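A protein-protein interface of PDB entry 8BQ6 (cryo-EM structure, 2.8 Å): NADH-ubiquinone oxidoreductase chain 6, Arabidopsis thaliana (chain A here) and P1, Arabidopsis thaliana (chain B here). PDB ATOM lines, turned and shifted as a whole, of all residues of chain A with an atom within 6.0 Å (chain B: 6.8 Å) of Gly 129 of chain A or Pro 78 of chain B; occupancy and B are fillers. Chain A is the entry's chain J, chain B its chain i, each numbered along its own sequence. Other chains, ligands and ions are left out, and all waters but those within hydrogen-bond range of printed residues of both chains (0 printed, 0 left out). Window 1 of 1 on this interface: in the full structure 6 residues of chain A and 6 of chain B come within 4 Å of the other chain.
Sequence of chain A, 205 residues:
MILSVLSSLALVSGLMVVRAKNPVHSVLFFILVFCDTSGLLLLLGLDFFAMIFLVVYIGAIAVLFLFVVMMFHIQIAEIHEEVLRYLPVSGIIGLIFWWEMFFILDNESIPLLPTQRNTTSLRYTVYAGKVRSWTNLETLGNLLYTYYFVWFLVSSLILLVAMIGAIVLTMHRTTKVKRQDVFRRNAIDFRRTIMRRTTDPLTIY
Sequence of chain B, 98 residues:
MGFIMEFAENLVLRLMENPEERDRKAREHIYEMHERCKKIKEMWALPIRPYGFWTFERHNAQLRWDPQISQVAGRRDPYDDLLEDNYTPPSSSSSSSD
Among the printed residues, merely in contact across the chains: Val 126 of chain A with Tyr 79 of chain B, Ala 128 of chain A with Pro 78 of chain B, Ala 128 of chain A with Tyr 79 of chain B, Ala 128 of chain A with Leu 82 of chain B and Gly 129 of chain A with Pro 78 of chain B.
Of the printed residues of chain B, Gly 129 of chain A touches Pro 78 (3.97 Å). Of the printed residues of chain B, Val 126 of chain A touches Tyr 79. Of the printed residues of chain A, Tyr 79 of chain B touches Val 126 (3.97 Å) and Ala 128 (3.9 Å).
Hydrophobic or aromatic side chains of chain A that line the printed part of chain B: Val 126 and Ala 128. Of the 8 printed residues of chain B, 3 touch a printed residue of chain A. Hydrophobic or aromatic side chains of chain B that line the printed part of chain A: Pro 78, Tyr 79 and Leu 82. Along chain B the printed residues that touch a printed residue of chain A span positions 78 to 82.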
ATOM      1  N   VAL A 126      -1.157 -22.922  28.466  1.00  0.00           N
ATOM      2  CA  VAL A 126      -2.120 -23.628  27.629  1.00  0.00           C
ATOM      3  C   VAL A 126      -2.964 -22.575  26.926  1.00  0.00           C
ATOM      4  O   VAL A 126      -3.805 -21.920  27.552  1.00  0.00           O
ATOM      5  CB  VAL A 126      -2.997 -24.588  28.443  1.00  0.00           C
ATOM      6  CG1 VAL A 126      -4.036 -25.237  27.549  1.00  0.00           C
ATOM      7  CG2 VAL A 126      -2.141 -25.640  29.117  1.00  0.00           C
ATOM      8  N   TYR A 127      -2.754 -22.415  25.621  1.00  0.00           N
ATOM      9  CA  TYR A 127      -3.422 -21.341  24.902  1.00  0.00           C
ATOM     10  C   TYR A 127      -4.892 -21.627  24.629  1.00  0.00           C
ATOM     11  O   TYR A 127      -5.638 -20.692  24.323  1.00  0.00           O
ATOM     12  CB  TYR A 127      -2.714 -21.067  23.579  1.00  0.00           C
ATOM     13  CG  TYR A 127      -1.326 -20.509  23.699  1.00  0.00           C
ATOM     14  CD1 TYR A 127      -1.121 -19.154  23.907  1.00  0.00           C
ATOM     15  CD2 TYR A 127      -0.217 -21.330  23.575  1.00  0.00           C
ATOM     16  CE1 TYR A 127       0.148 -18.636  24.008  1.00  0.00           C
ATOM     17  CE2 TYR A 127       1.055 -20.821  23.674  1.00  0.00           C
ATOM     18  CZ  TYR A 127       1.233 -19.474  23.891  1.00  0.00           C
ATOM     19  OH  TYR A 127       2.503 -18.960  23.990  1.00  0.00           O
ATOM     20  N   ALA A 128      -5.323 -22.886  24.730  1.00  0.00           N
ATOM     21  CA  ALA A 128      -6.712 -23.216  24.428  1.00  0.00           C
ATOM     22  C   ALA A 128      -7.671 -22.490  25.361  1.00  0.00           C
ATOM     23  O   ALA A 128      -8.733 -22.023  24.932  1.00  0.00           O
ATOM     24  CB  ALA A 128      -6.923 -24.727  24.512  1.00  0.00           C
ATOM     25  N   GLY A 129      -7.318 -22.378  26.637  1.00  0.00           N
ATOM     26  CA  GLY A 129      -8.152 -21.639  27.563  1.00  0.00           C
ATOM     27  C   GLY A 129      -8.231 -20.147  27.313  1.00  0.00           C
ATOM     28  O   GLY A 129      -9.131 -19.495  27.848  1.00  0.00           O
ATOM     29  N   LYS A 130      -7.326 -19.591  26.509  1.00  0.00           N
ATOM     30  CA  LYS A 130      -7.212 -18.151  26.317  1.00  0.00           C
ATOM     31  C   LYS A 130      -7.915 -17.638  25.068  1.00  0.00           C
ATOM     32  O   LYS A 130      -7.854 -16.435  24.801  1.00  0.00           O
ATOM     33  CB  LYS A 130      -5.741 -17.752  26.246  1.00  0.00           C
ATOM     34  CG  LYS A 130      -5.044 -17.687  27.570  1.00  0.00           C
ATOM     35  CD  LYS A 130      -3.549 -17.667  27.369  1.00  0.00           C
ATOM     36  CE  LYS A 130      -2.844 -17.418  28.681  1.00  0.00           C
ATOM     37  NZ  LYS A 130      -3.149 -18.498  29.657  1.00  0.00           N
ATOM     38  N   VAL A 131      -8.553 -18.511  24.288  1.00  0.00           N
ATOM     39  CA  VAL A 131      -9.178 -18.072  23.043  1.00  0.00           C
ATOM     40  C   VAL A 131     -10.353 -17.144  23.325  1.00  0.00           C
ATOM     41  O   VAL A 131     -10.458 -16.056  22.745  1.00  0.00           O
ATOM     42  CB  VAL A 131      -9.613 -19.291  22.211  1.00  0.00           C
ATOM     43  CG1 VAL A 131     -10.548 -18.863  21.097  1.00  0.00           C
ATOM     44  CG2 VAL A 131      -8.404 -20.004  21.643  1.00  0.00           C
ATOM     45  N   ARG A 132     -11.259 -17.565  24.208  1.00  0.00           N
ATOM     46  CA  ARG A 132     -12.418 -16.776  24.635  1.00  0.00           C
ATOM     47  C   ARG A 132     -12.473 -16.908  26.153  1.00  0.00           C
ATOM     48  O   ARG A 132     -13.086 -17.838  26.683  1.00  0.00           O
ATOM     49  CB  ARG A 132     -13.710 -17.256  23.980  1.00  0.00           C
ATOM     50  CG  ARG A 132     -14.961 -16.496  24.426  1.00  0.00           C
ATOM     51  CD  ARG A 132     -16.231 -17.068  23.799  1.00  0.00           C
ATOM     52  NE  ARG A 132     -17.437 -16.407  24.287  1.00  0.00           N
ATOM     53  CZ  ARG A 132     -18.645 -16.577  23.766  1.00  0.00           C
ATOM     54  NH1 ARG A 132     -18.852 -17.405  22.755  1.00  0.00           N
ATOM     55  NH2 ARG A 132     -19.670 -15.891  24.265  1.00  0.00           N
ATOM     56  N   SER A 133     -11.821 -15.981  26.846  1.00  0.00           N
ATOM     57  CA  SER A 133     -11.794 -16.006  28.301  1.00  0.00           C
ATOM     58  C   SER A 133     -13.027 -15.329  28.884  1.00  0.00           C
ATOM     59  O   SER A 133     -13.628 -14.450  28.260  1.00  0.00           O
ATOM     60  CB  SER A 133     -10.541 -15.316  28.814  1.00  0.00           C
ATOM     61  OG  SER A 133     -10.364 -14.067  28.163  1.00  0.00           O
ATOM     62  N   ARG B  76     -16.388 -27.123  30.641  1.00  0.00           N
ATOM     63  CA  ARG B  76     -15.838 -27.998  29.619  1.00  0.00           C
ATOM     64  C   ARG B  76     -14.320 -27.998  29.652  1.00  0.00           C
ATOM     65  O   ARG B  76     -13.682 -27.012  30.029  1.00  0.00           O
ATOM     66  CB  ARG B  76     -16.307 -27.567  28.234  1.00  0.00           C
ATOM     67  CG  ARG B  76     -17.781 -27.339  28.182  1.00  0.00           C
ATOM     68  CD  ARG B  76     -18.259 -27.183  26.778  1.00  0.00           C
ATOM     69  NE  ARG B  76     -18.083 -28.402  26.004  1.00  0.00           N
ATOM     70  CZ  ARG B  76     -18.221 -28.462  24.689  1.00  0.00           C
ATOM     71  NH1 ARG B  76     -18.573 -27.400  23.985  1.00  0.00           N
ATOM     72  NH2 ARG B  76     -18.010 -29.616  24.064  1.00  0.00           N
ATOM     73  N   ASP B  77     -13.749 -29.124  29.249  1.00  0.00           N
ATOM     74  CA  ASP B  77     -12.341 -29.155  28.899  1.00  0.00           C
ATOM     75  C   ASP B  77     -12.105 -28.156  27.771  1.00  0.00           C
ATOM     76  O   ASP B  77     -12.894 -28.110  26.818  1.00  0.00           O
ATOM     77  CB  ASP B  77     -11.945 -30.573  28.481  1.00  0.00           C
ATOM     78  CG  ASP B  77     -10.461 -30.723  28.187  1.00  0.00           C
ATOM     79  OD1 ASP B  77      -9.696 -29.745  28.316  1.00  0.00           O
ATOM     80  OD2 ASP B  77     -10.053 -31.846  27.828  1.00  0.00           O
ATOM     81  N   PRO B  78     -11.071 -27.316  27.859  1.00  0.00           N
ATOM     82  CA  PRO B  78     -10.875 -26.288  26.822  1.00  0.00           C
ATOM     83  C   PRO B  78     -10.684 -26.838  25.418  1.00  0.00           C
ATOM     84  O   PRO B  78     -11.040 -26.156  24.451  1.00  0.00           O
ATOM     85  CB  PRO B  78      -9.630 -25.533  27.312  1.00  0.00           C
ATOM     86  CG  PRO B  78      -9.003 -26.422  28.346  1.00  0.00           C
ATOM     87  CD  PRO B  78     -10.138 -27.144  28.982  1.00  0.00           C
ATOM     88  N   TYR B  79     -10.137 -28.045  25.266  1.00  0.00           N
ATOM     89  CA  TYR B  79      -9.922 -28.581  23.926  1.00  0.00           C
ATOM     90  C   TYR B  79     -11.220 -28.972  23.234  1.00  0.00           C
ATOM     91  O   TYR B  79     -11.227 -29.133  22.009  1.00  0.00           O
ATOM     92  CB  TYR B  79      -8.965 -29.770  23.990  1.00  0.00           C
ATOM     93  CG  TYR B  79      -7.542 -29.325  24.195  1.00  0.00           C
ATOM     94  CD1 TYR B  79      -6.859 -28.663  23.188  1.00  0.00           C
ATOM     95  CD2 TYR B  79      -6.896 -29.519  25.408  1.00  0.00           C
ATOM     96  CE1 TYR B  79      -5.569 -28.232  23.367  1.00  0.00           C
ATOM     97  CE2 TYR B  79      -5.599 -29.087  25.597  1.00  0.00           C
ATOM     98  CZ  TYR B  79      -4.942 -28.444  24.570  1.00  0.00           C
ATOM     99  OH  TYR B  79      -3.651 -28.007  24.738  1.00  0.00           O
ATOM    100  N   ASP B  80     -12.317 -29.107  23.982  1.00  0.00           N
ATOM    101  CA  ASP B  80     -13.583 -29.517  23.383  1.00  0.00           C
ATOM    102  C   ASP B  80     -14.099 -28.497  22.382  1.00  0.00           C
ATOM    103  O   ASP B  80     -14.761 -28.865  21.407  1.00  0.00           O
ATOM    104  CB  ASP B  80     -14.626 -29.744  24.471  1.00  0.00           C
ATOM    105  CG  ASP B  80     -14.350 -30.981  25.286  1.00  0.00           C
ATOM    106  OD1 ASP B  80     -14.185 -32.061  24.687  1.00  0.00           O
ATOM    107  OD2 ASP B  80     -14.312 -30.880  26.525  1.00  0.00           O
ATOM    108  N   ASP B  81     -13.829 -27.214  22.615  1.00  0.00           N
ATOM    109  CA  ASP B  81     -14.283 -26.193  21.681  1.00  0.00           C
ATOM    110  C   ASP B  81     -13.470 -26.225  20.395  1.00  0.00           C
ATOM    111  O   ASP B  81     -13.976 -25.870  19.323  1.00  0.00           O
ATOM    112  CB  ASP B  81     -14.197 -24.817  22.336  1.00  0.00           C
ATOM    113  CG  ASP B  81     -15.516 -24.372  22.921  1.00  0.00           C
ATOM    114  OD1 ASP B  81     -15.588 -23.228  23.415  1.00  0.00           O
ATOM    115  OD2 ASP B  81     -16.478 -25.168  22.890  1.00  0.00           O
ATOM    116  N   LEU B  82     -12.207 -26.647  20.481  1.00  0.00           N
ATOM    117  CA  LEU B  82     -11.345 -26.635  19.305  1.00  0.00           C
ATOM    118  C   LEU B  82     -11.686 -27.756  18.336  1.00  0.00           C
ATOM    119  O   LEU B  82     -11.460 -27.619  17.129  1.00  0.00           O
ATOM    120  CB  LEU B  82      -9.876 -26.728  19.718  1.00  0.00           C
ATOM    121  CG  LEU B  82      -9.294 -25.561  20.520  1.00  0.00           C
ATOM    122  CD1 LEU B  82      -7.876 -25.879  20.972  1.00  0.00           C
ATOM    123  CD2 LEU B  82      -9.347 -24.255  19.763  1.00  0.00           C
ATOM    124  N   LEU B  83     -12.217 -28.867  18.838  1.00  0.00           N
ATOM    125  CA  LEU B  83     -12.561 -30.008  18.006  1.00  0.00           C
ATOM    126  C   LEU B  83     -14.036 -30.051  17.637  1.00  0.00           C
ATOM    127  O   LEU B  83     -14.404 -30.777  16.707  1.00  0.00           O
ATOM    128  CB  LEU B  83     -12.169 -31.307  18.717  1.00  0.00           C
ATOM    129  CG  LEU B  83     -10.656 -31.476  18.866  1.00  0.00           C
ATOM    130  CD1 LEU B  83     -10.318 -32.693  19.689  1.00  0.00           C
ATOM    131  CD2 LEU B  83     -10.017 -31.578  17.500  1.00  0.00           C
